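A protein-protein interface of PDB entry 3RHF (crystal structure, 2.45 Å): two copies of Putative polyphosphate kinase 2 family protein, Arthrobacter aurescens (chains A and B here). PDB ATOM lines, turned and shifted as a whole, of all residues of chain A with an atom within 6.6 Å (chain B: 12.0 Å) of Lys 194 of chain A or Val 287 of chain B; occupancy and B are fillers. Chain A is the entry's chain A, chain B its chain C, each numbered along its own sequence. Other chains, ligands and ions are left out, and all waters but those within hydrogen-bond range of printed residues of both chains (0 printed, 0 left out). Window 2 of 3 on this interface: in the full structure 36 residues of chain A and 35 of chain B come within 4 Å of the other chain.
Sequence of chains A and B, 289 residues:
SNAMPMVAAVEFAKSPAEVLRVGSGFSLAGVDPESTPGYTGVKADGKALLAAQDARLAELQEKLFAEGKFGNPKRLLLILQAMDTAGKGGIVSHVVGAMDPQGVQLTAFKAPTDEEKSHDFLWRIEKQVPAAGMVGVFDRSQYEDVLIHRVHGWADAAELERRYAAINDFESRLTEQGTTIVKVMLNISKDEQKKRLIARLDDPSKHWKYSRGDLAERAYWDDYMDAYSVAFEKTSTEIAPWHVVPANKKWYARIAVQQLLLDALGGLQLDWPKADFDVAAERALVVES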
ATOM      1  N   THR A  85     -13.098  25.064  -1.840  1.00  0.00           N
ATOM      2  CA  THR A  85     -14.490  24.702  -2.031  1.00  0.00           C
ATOM      3  C   THR A  85     -15.427  25.549  -1.160  1.00  0.00           C
ATOM      4  O   THR A  85     -16.609  25.677  -1.479  1.00  0.00           O
ATOM      5  CB  THR A  85     -14.620  23.156  -1.744  1.00  0.00           C
ATOM      6  OG1 THR A  85     -14.759  22.462  -2.990  1.00  0.00           O
ATOM      7  CG2 THR A  85     -15.692  22.836  -0.801  1.00  0.00           C
ATOM      8  N   ILE A 188     -17.184  25.298   6.335  1.00  0.00           N
ATOM      9  CA  ILE A 188     -18.028  24.237   5.798  1.00  0.00           C
ATOM     10  C   ILE A 188     -17.661  22.950   6.483  1.00  0.00           C
ATOM     11  O   ILE A 188     -16.537  22.802   6.994  1.00  0.00           O
ATOM     12  CB  ILE A 188     -17.931  24.092   4.270  1.00  0.00           C
ATOM     13  CG1 ILE A 188     -16.493  23.739   3.824  1.00  0.00           C
ATOM     14  CG2 ILE A 188     -18.472  25.387   3.605  1.00  0.00           C
ATOM     15  CD1 ILE A 188     -16.318  23.562   2.317  1.00  0.00           C
ATOM     16  N   SER A 189     -18.627  22.040   6.521  1.00  0.00           N
ATOM     17  CA  SER A 189     -18.422  20.707   7.087  1.00  0.00           C
ATOM     18  C   SER A 189     -17.569  19.857   6.158  1.00  0.00           C
ATOM     19  O   SER A 189     -17.553  20.076   4.942  1.00  0.00           O
ATOM     20  CB  SER A 189     -19.754  20.020   7.318  1.00  0.00           C
ATOM     21  OG  SER A 189     -20.338  19.680   6.089  1.00  0.00           O
ATOM     22  N   LYS A 190     -16.832  18.900   6.731  1.00  0.00           N
ATOM     23  CA  LYS A 190     -16.057  17.921   5.912  1.00  0.00           C
ATOM     24  C   LYS A 190     -16.923  17.240   4.834  1.00  0.00           C
ATOM     25  O   LYS A 190     -16.456  17.019   3.725  1.00  0.00           O
ATOM     26  CB  LYS A 190     -15.335  16.874   6.774  1.00  0.00           C
ATOM     27  CG  LYS A 190     -14.177  16.114   6.038  1.00  0.00           C
ATOM     28  CD  LYS A 190     -13.712  14.880   6.815  1.00  0.00           C
ATOM     29  CE  LYS A 190     -12.442  14.220   6.201  1.00  0.00           C
ATOM     30  NZ  LYS A 190     -11.815  13.090   7.007  1.00  0.00           N
ATOM     31  N   ASP A 191     -18.195  16.988   5.107  1.00  0.00           N
ATOM     32  CA  ASP A 191     -19.049  16.405   4.058  1.00  0.00           C
ATOM     33  C   ASP A 191     -19.447  17.346   2.938  1.00  0.00           C
ATOM     34  O   ASP A 191     -19.506  16.937   1.773  1.00  0.00           O
ATOM     35  CB  ASP A 191     -20.320  15.826   4.666  1.00  0.00           C
ATOM     36  CG  ASP A 191     -20.072  14.538   5.392  1.00  0.00           C
ATOM     37  OD1 ASP A 191     -19.020  13.871   5.075  1.00  0.00           O
ATOM     38  OD2 ASP A 191     -20.937  14.235   6.270  1.00  0.00           O
ATOM     39  N   GLU A 192     -19.760  18.591   3.299  1.00  0.00           N
ATOM     40  CA  GLU A 192     -19.989  19.651   2.306  1.00  0.00           C
ATOM     41  C   GLU A 192     -18.822  19.774   1.317  1.00  0.00           C
ATOM     42  O   GLU A 192     -19.055  19.936   0.119  1.00  0.00           O
ATOM     43  CB  GLU A 192     -20.249  21.005   2.976  1.00  0.00           C
ATOM     44  CG  GLU A 192     -20.810  22.079   2.042  1.00  0.00           C
ATOM     45  CD  GLU A 192     -22.143  21.718   1.384  1.00  0.00           C
ATOM     46  OE1 GLU A 192     -22.970  21.014   1.997  1.00  0.00           O
ATOM     47  OE2 GLU A 192     -22.364  22.148   0.238  1.00  0.00           O
ATOM     48  N   GLN A 193     -17.584  19.693   1.806  1.00  0.00           N
ATOM     49  CA  GLN A 193     -16.449  19.744   0.896  1.00  0.00           C
ATOM     50  C   GLN A 193     -16.511  18.580  -0.110  1.00  0.00           C
ATOM     51  O   GLN A 193     -16.307  18.761  -1.320  1.00  0.00           O
ATOM     52  CB  GLN A 193     -15.149  19.658   1.658  1.00  0.00           C
ATOM     53  CG  GLN A 193     -14.078  20.433   1.078  1.00  0.00           C
ATOM     54  CD  GLN A 193     -12.784  19.687   0.892  1.00  0.00           C
ATOM     55  OE1 GLN A 193     -12.795  18.493   0.657  1.00  0.00           O
ATOM     56  NE2 GLN A 193     -11.646  20.432   0.893  1.00  0.00           N
ATOM     57  N   LYS A 194     -16.786  17.390   0.413  1.00  0.00           N
ATOM     58  CA  LYS A 194     -16.927  16.190  -0.407  1.00  0.00           C
ATOM     59  C   LYS A 194     -18.024  16.388  -1.447  1.00  0.00           C
ATOM     60  O   LYS A 194     -17.816  16.137  -2.624  1.00  0.00           O
ATOM     61  CB  LYS A 194     -17.173  14.946   0.466  1.00  0.00           C
ATOM     62  CG  LYS A 194     -17.610  13.724  -0.312  1.00  0.00           C
ATOM     63  CD  LYS A 194     -17.135  12.372   0.292  1.00  0.00           C
ATOM     64  CE  LYS A 194     -17.769  12.005   1.631  1.00  0.00           C
ATOM     65  NZ  LYS A 194     -17.339  10.602   2.048  1.00  0.00           N
ATOM     66  N   LYS A 195     -19.174  16.875  -1.005  1.00  0.00           N
ATOM     67  CA  LYS A 195     -20.281  17.167  -1.911  1.00  0.00           C
ATOM     68  C   LYS A 195     -19.841  18.149  -3.004  1.00  0.00           C
ATOM     69  O   LYS A 195     -20.201  18.016  -4.164  1.00  0.00           O
ATOM     70  CB  LYS A 195     -21.441  17.735  -1.099  1.00  0.00           C
ATOM     71  CG  LYS A 195     -22.818  17.693  -1.784  1.00  0.00           C
ATOM     72  CD  LYS A 195     -23.891  18.558  -1.048  1.00  0.00           C
ATOM     73  CE  LYS A 195     -25.047  19.105  -1.967  1.00  0.00           C
ATOM     74  NZ  LYS A 195     -25.836  20.216  -1.261  1.00  0.00           N
ATOM     75  N   ARG A 196     -19.030  19.131  -2.634  1.00  0.00           N
ATOM     76  CA  ARG A 196     -18.588  20.117  -3.594  1.00  0.00           C
ATOM     77  C   ARG A 196     -17.548  19.571  -4.584  1.00  0.00           C
ATOM     78  O   ARG A 196     -17.637  19.885  -5.773  1.00  0.00           O
ATOM     79  CB  ARG A 196     -18.148  21.429  -2.906  1.00  0.00           C
ATOM     80  CG  ARG A 196     -19.344  22.146  -2.326  1.00  0.00           C
ATOM     81  CD  ARG A 196     -19.011  23.377  -1.533  1.00  0.00           C
ATOM     82  NE  ARG A 196     -20.184  23.883  -0.809  1.00  0.00           N
ATOM     83  CZ  ARG A 196     -20.241  25.064  -0.194  1.00  0.00           C
ATOM     84  NH1 ARG A 196     -19.213  25.901  -0.221  1.00  0.00           N
ATOM     85  NH2 ARG A 196     -21.292  25.400   0.490  1.00  0.00           N
ATOM     86  N   LEU A 197     -16.584  18.773  -4.126  1.00  0.00           N
ATOM     87  CA  LEU A 197     -15.593  18.217  -5.058  1.00  0.00           C
ATOM     88  C   LEU A 197     -16.275  17.260  -6.022  1.00  0.00           C
ATOM     89  O   LEU A 197     -15.959  17.235  -7.224  1.00  0.00           O
ATOM     90  CB  LEU A 197     -14.468  17.507  -4.337  1.00  0.00           C
ATOM     91  CG  LEU A 197     -13.512  18.376  -3.539  1.00  0.00           C
ATOM     92  CD1 LEU A 197     -12.676  17.477  -2.667  1.00  0.00           C
ATOM     93  CD2 LEU A 197     -12.633  19.226  -4.451  1.00  0.00           C
ATOM     94  N   ILE A 198     -17.235  16.498  -5.513  1.00  0.00           N
ATOM     95  CA  ILE A 198     -17.991  15.604  -6.377  1.00  0.00           C
ATOM     96  C   ILE A 198     -18.734  16.384  -7.443  1.00  0.00           C
ATOM     97  O   ILE A 198     -18.739  16.001  -8.605  1.00  0.00           O
ATOM     98  CB  ILE A 198     -18.996  14.754  -5.591  1.00  0.00           C
ATOM     99  CG1 ILE A 198     -18.297  13.590  -4.906  1.00  0.00           C
ATOM    100  CG2 ILE A 198     -20.067  14.186  -6.533  1.00  0.00           C
ATOM    101  CD1 ILE A 198     -19.209  12.886  -3.821  1.00  0.00           C
ATOM    102  N   ALA A 199     -19.372  17.484  -7.034  1.00  0.00           N
ATOM    103  CA  ALA A 199     -20.060  18.363  -8.006  1.00  0.00           C
ATOM    104  C   ALA A 199     -19.093  18.916  -9.073  1.00  0.00           C
ATOM    105  O   ALA A 199     -19.447  19.013 -10.248  1.00  0.00           O
ATOM    106  CB  ALA A 199     -20.852  19.455  -7.320  1.00  0.00           C
ATOM    107  N   LEU A 215      -8.155  16.813  -2.622  1.00  0.00           N
ATOM    108  CA  LEU A 215      -8.447  15.493  -2.094  1.00  0.00           C
ATOM    109  C   LEU A 215      -7.331  15.096  -1.092  1.00  0.00           C
ATOM    110  O   LEU A 215      -7.623  14.690   0.038  1.00  0.00           O
ATOM    111  CB  LEU A 215      -8.595  14.479  -3.244  1.00  0.00           C
ATOM    112  CG  LEU A 215      -8.824  13.006  -2.899  1.00  0.00           C
ATOM    113  CD1 LEU A 215     -10.011  12.869  -1.954  1.00  0.00           C
ATOM    114  CD2 LEU A 215      -9.032  12.187  -4.146  1.00  0.00           C
ATOM    115  N   ARG A 218      -7.857  16.502   2.418  1.00  0.00           N
ATOM    116  CA  ARG A 218      -8.967  15.989   3.244  1.00  0.00           C
ATOM    117  C   ARG A 218      -8.424  15.070   4.335  1.00  0.00           C
ATOM    118  O   ARG A 218      -8.948  15.018   5.444  1.00  0.00           O
ATOM    119  CB  ARG A 218     -10.002  15.203   2.425  1.00  0.00           C
ATOM    120  CG  ARG A 218     -10.894  16.024   1.536  1.00  0.00           C
ATOM    121  CD  ARG A 218     -11.898  15.167   0.742  1.00  0.00           C
ATOM    122  NE  ARG A 218     -12.820  14.391   1.590  1.00  0.00           N
ATOM    123  CZ  ARG A 218     -13.809  14.909   2.325  1.00  0.00           C
ATOM    124  NH1 ARG A 218     -14.583  14.112   3.049  1.00  0.00           N
ATOM    125  NH2 ARG A 218     -14.048  16.219   2.344  1.00  0.00           N
ATOM    126  N   PHE B 277      -7.563  13.357 -17.299  1.00  0.00           N
ATOM    127  CA  PHE B 277      -7.506  12.294 -16.288  1.00  0.00           C
ATOM    128  C   PHE B 277      -8.855  11.578 -16.184  1.00  0.00           C
ATOM    129  O   PHE B 277      -9.890  12.095 -16.602  1.00  0.00           O
ATOM    130  CB  PHE B 277      -7.109  12.840 -14.903  1.00  0.00           C
ATOM    131  CG  PHE B 277      -8.109  13.792 -14.321  1.00  0.00           C
ATOM    132  CD1 PHE B 277      -9.282  13.322 -13.749  1.00  0.00           C
ATOM    133  CD2 PHE B 277      -7.899  15.160 -14.374  1.00  0.00           C
ATOM    134  CE1 PHE B 277     -10.214  14.193 -13.237  1.00  0.00           C
ATOM    135  CE2 PHE B 277      -8.835  16.048 -13.858  1.00  0.00           C
ATOM    136  CZ  PHE B 277      -9.986  15.568 -13.291  1.00  0.00           C
ATOM    137  N   ASP B 278      -8.833  10.395 -15.582  1.00  0.00           N
ATOM    138  CA  ASP B 278     -10.031   9.558 -15.456  1.00  0.00           C
ATOM    139  C   ASP B 278     -10.973  10.176 -14.421  1.00  0.00           C
ATOM    140  O   ASP B 278     -10.804  10.038 -13.203  1.00  0.00           O
ATOM    141  CB  ASP B 278      -9.655   8.087 -15.121  1.00  0.00           C
ATOM    142  CG  ASP B 278     -10.860   7.097 -15.185  1.00  0.00           C
ATOM    143  OD1 ASP B 278     -12.040   7.536 -15.392  1.00  0.00           O
ATOM    144  OD2 ASP B 278     -10.600   5.862 -15.005  1.00  0.00           O
ATOM    145  N   VAL B 279     -11.961  10.880 -14.948  1.00  0.00           N
ATOM    146  CA  VAL B 279     -12.976  11.489 -14.122  1.00  0.00           C
ATOM    147  C   VAL B 279     -13.628  10.440 -13.217  1.00  0.00           C
ATOM    148  O   VAL B 279     -13.788  10.662 -12.017  1.00  0.00           O
ATOM    149  CB  VAL B 279     -14.042  12.200 -14.968  1.00  0.00           C
ATOM    150  CG1 VAL B 279     -15.022  12.969 -14.059  1.00  0.00           C
ATOM    151  CG2 VAL B 279     -13.373  13.150 -15.971  1.00  0.00           C
ATOM    152  N   ALA B 280     -13.964   9.286 -13.778  1.00  0.00           N
ATOM    153  CA  ALA B 280     -14.706   8.278 -13.024  1.00  0.00           C
ATOM    154  C   ALA B 280     -13.895   7.717 -11.858  1.00  0.00           C
ATOM    155  O   ALA B 280     -14.432   7.491 -10.751  1.00  0.00           O
ATOM    156  CB  ALA B 280     -15.203   7.165 -13.959  1.00  0.00           C
ATOM    157  N   ALA B 281     -12.603   7.527 -12.099  1.00  0.00           N
ATOM    158  CA  ALA B 281     -11.705   6.979 -11.073  1.00  0.00           C
ATOM    159  C   ALA B 281     -11.569   7.993  -9.937  1.00  0.00           C
ATOM    160  O   ALA B 281     -11.752   7.666  -8.752  1.00  0.00           O
ATOM    161  CB  ALA B 281     -10.298   6.596 -11.657  1.00  0.00           C
ATOM    162  N   GLU B 282     -11.279   9.230 -10.300  1.00  0.00           N
ATOM    163  CA  GLU B 282     -11.156  10.274  -9.293  1.00  0.00           C
ATOM    164  C   GLU B 282     -12.448  10.378  -8.475  1.00  0.00           C
ATOM    165  O   GLU B 282     -12.400  10.390  -7.247  1.00  0.00           O
ATOM    166  CB  GLU B 282     -10.783  11.610  -9.944  1.00  0.00           C
ATOM    167  CG  GLU B 282     -10.116  12.594  -9.012  1.00  0.00           C
ATOM    168  CD  GLU B 282      -8.677  12.273  -8.748  1.00  0.00           C
ATOM    169  OE1 GLU B 282      -8.151  11.273  -9.306  1.00  0.00           O
ATOM    170  OE2 GLU B 282      -8.078  13.023  -7.949  1.00  0.00           O
ATOM    171  N   ARG B 283     -13.604  10.390  -9.137  1.00  0.00           N
ATOM    172  CA  ARG B 283     -14.886  10.479  -8.410  1.00  0.00           C
ATOM    173  C   ARG B 283     -15.003   9.379  -7.337  1.00  0.00           C
ATOM    174  O   ARG B 283     -15.394   9.654  -6.198  1.00  0.00           O
ATOM    175  CB  ARG B 283     -16.061  10.422  -9.388  1.00  0.00           C
ATOM    176  CG  ARG B 283     -17.430  10.592  -8.768  1.00  0.00           C
ATOM    177  CD  ARG B 283     -18.563  10.365  -9.765  1.00  0.00           C
ATOM    178  NE  ARG B 283     -19.779  11.066  -9.351  1.00  0.00           N
ATOM    179  CZ  ARG B 283     -20.562  10.703  -8.330  1.00  0.00           C
ATOM    180  NH1 ARG B 283     -20.313   9.621  -7.592  1.00  0.00           N
ATOM    181  NH2 ARG B 283     -21.628  11.430  -8.050  1.00  0.00           N
ATOM    182  N   ALA B 284     -14.658   8.141  -7.711  1.00  0.00           N
ATOM    183  CA  ALA B 284     -14.679   6.988  -6.796  1.00  0.00           C
ATOM    184  C   ALA B 284     -13.747   7.207  -5.637  1.00  0.00           C
ATOM    185  O   ALA B 284     -14.085   6.969  -4.497  1.00  0.00           O
ATOM    186  CB  ALA B 284     -14.269   5.728  -7.530  1.00  0.00           C
ATOM    187  N   LEU B 285     -12.556   7.666  -5.960  1.00  0.00           N
ATOM    188  CA  LEU B 285     -11.547   8.019  -4.971  1.00  0.00           C
ATOM    189  C   LEU B 285     -12.095   9.103  -4.015  1.00  0.00           C
ATOM    190  O   LEU B 285     -11.857   9.066  -2.784  1.00  0.00           O
ATOM    191  CB  LEU B 285     -10.272   8.491  -5.704  1.00  0.00           C
ATOM    192  CG  LEU B 285      -8.903   7.851  -5.417  1.00  0.00           C
ATOM    193  CD1 LEU B 285      -8.919   6.306  -5.229  1.00  0.00           C
ATOM    194  CD2 LEU B 285      -7.932   8.281  -6.533  1.00  0.00           C
ATOM    195  N   VAL B 286     -12.849  10.059  -4.560  1.00  0.00           N
ATOM    196  CA  VAL B 286     -13.415  11.111  -3.698  1.00  0.00           C
ATOM    197  C   VAL B 286     -14.514  10.514  -2.834  1.00  0.00           C
ATOM    198  O   VAL B 286     -14.615  10.847  -1.647  1.00  0.00           O
ATOM    199  CB  VAL B 286     -13.898  12.395  -4.457  1.00  0.00           C
ATOM    200  CG1 VAL B 286     -14.488  13.401  -3.482  1.00  0.00           C
ATOM    201  CG2 VAL B 286     -12.761  13.050  -5.188  1.00  0.00           C
ATOM    202  N   VAL B 287     -15.304   9.618  -3.408  1.00  0.00           N
ATOM    203  CA  VAL B 287     -16.410   9.033  -2.684  1.00  0.00           C
ATOM    204  C   VAL B 287     -15.920   8.288  -1.443  1.00  0.00           C
ATOM    205  O   VAL B 287     -16.586   8.319  -0.418  1.00  0.00           O
ATOM    206  CB  VAL B 287     -17.257   8.133  -3.608  1.00  0.00           C
ATOM    207  CG1 VAL B 287     -17.905   6.993  -2.849  1.00  0.00           C
ATOM    208  CG2 VAL B 287     -18.323   8.974  -4.335  1.00  0.00           C
ATOM    209  N   GLU B 288     -14.744   7.666  -1.535  1.00  0.00           N
ATOM    210  CA  GLU B 288     -14.158   6.842  -0.443  1.00  0.00           C
ATOM    211  C   GLU B 288     -13.423   7.658   0.622  1.00  0.00           C
ATOM    212  O   GLU B 288     -13.241   7.161   1.735  1.00  0.00           O
ATOM    213  CB  GLU B 288     -13.176   5.782  -0.982  1.00  0.00           C
ATOM    214  CG  GLU B 288     -13.749   4.733  -1.992  1.00  0.00           C
ATOM    215  CD  GLU B 288     -15.041   3.976  -1.515  1.00  0.00           C
ATOM    216  OE1 GLU B 288     -15.113   3.477  -0.345  1.00  0.00           O
ATOM    217  OE2 GLU B 288     -15.980   3.862  -2.348  1.00  0.00           O
ATOM    218  N   SER B 289     -12.955   8.864   0.264  1.00  0.00           N
ATOM    219  CA  SER B 289     -12.518   9.887   1.253  1.00  0.00           C
ATOM    220  C   SER B 289     -13.710  10.403   2.093  1.00  0.00           C
ATOM    221  O   SER B 289     -13.519  11.150   3.054  1.00  0.00           O
ATOM    222  CB  SER B 289     -11.802  11.091   0.552  1.00  0.00           C
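No residue of chain B comes within 4 Å of Gln 193 of chain A.
Lys 194 of chain A touches three residues of chain B.
Of chain B, only Arg 283 comes within 4 Å of Ile 198 of chain A.
Printed residues of chain B within 4 Å of Leu 215 of chain A: Val 286 and Ser 289.
Printed residues of chain B within 4 Å of Arg 218 of chain A: Ser 289 (3.1 Å).
Of the printed residues of chain A, Val 286 of chain B touches Lys 194 (3.5 Å) and Leu 215 (3.97 Å).
Val 287 of chain B touches just one residue of chain A: Lys 194 (3.4 Å).
Of the printed residues of chain A, Ser 289 of chain B touches Lys 194, Leu 215 and Arg 218.
The nearest residue of chain A that does not touch Val 287 of chain B is Ile 198 of chain A (4.04 Å).
The nearest printed residue of chain A that does not touch Val 286 of chain B is Ile 198 of chain A (4.1 Å).
No position is printed for both chains.
Of the 7 pairs that touch across the chains among the printed residues, none has its exchanged pair printed and touching as well.
The backbone carbonyl oxygen (O) of Lys 190 of chain A sits at hydrogen-bond distance from the guanidinium group (NH2) of Arg 218 of chain A (2.9 Å).
OE1 of Gln 193 of chain A lies within hydrogen-bond range of NH2 of Arg 218 of chain A.
CD of Lys 194 of chain A touches O of Val 286 of chain B (3.5 Å).
Lys 194 of chain A touches Ser 289 of chain B.
Ile 198 of chain A touches Arg 283 of chain B.
Val 286 of chain B touches Leu 215 of chain A (CG2 to CD2, 3.97 Å).
CB of Ser 289 of chain B touches CD1 of Leu 215 of chain A, at 3.6 Å.
Of the 13 printed residues of chain B, 4 touch a printed residue of chain A.
Printed residues of chain B that touch a printed residue of chain A: Arg 283, Val 286, Val 287 and Ser 289.
Hydrophobic or aromatic side chains of chain B within 4 Å of the printed part of chain A: Val 286.
Hydrophobic or aromatic side chains of chain A within 4 Å of the printed part of chain B: Ile 198 and Leu 215.
Along chain A the printed residues that touch a printed residue of chain B span positions 194 to 218.
Among the printed residues, 7 pairs touch across the chains.
Among the printed residues, no Asp or Glu carboxylate lies within 4 Å of a Lys or Arg side-chain nitrogen of the other chain.
The side-chain amino group (NZ) of Lys 194 of chain A lies within hydrogen-bond range of the backbone carbonyl oxygen (O) of Val 287 of chain B (3.4 Å).
The guanidinium group of Arg 218 of chain A is in hydrogen-bond range of the backbone carbonyl oxygen of Ser 289 of chain B.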
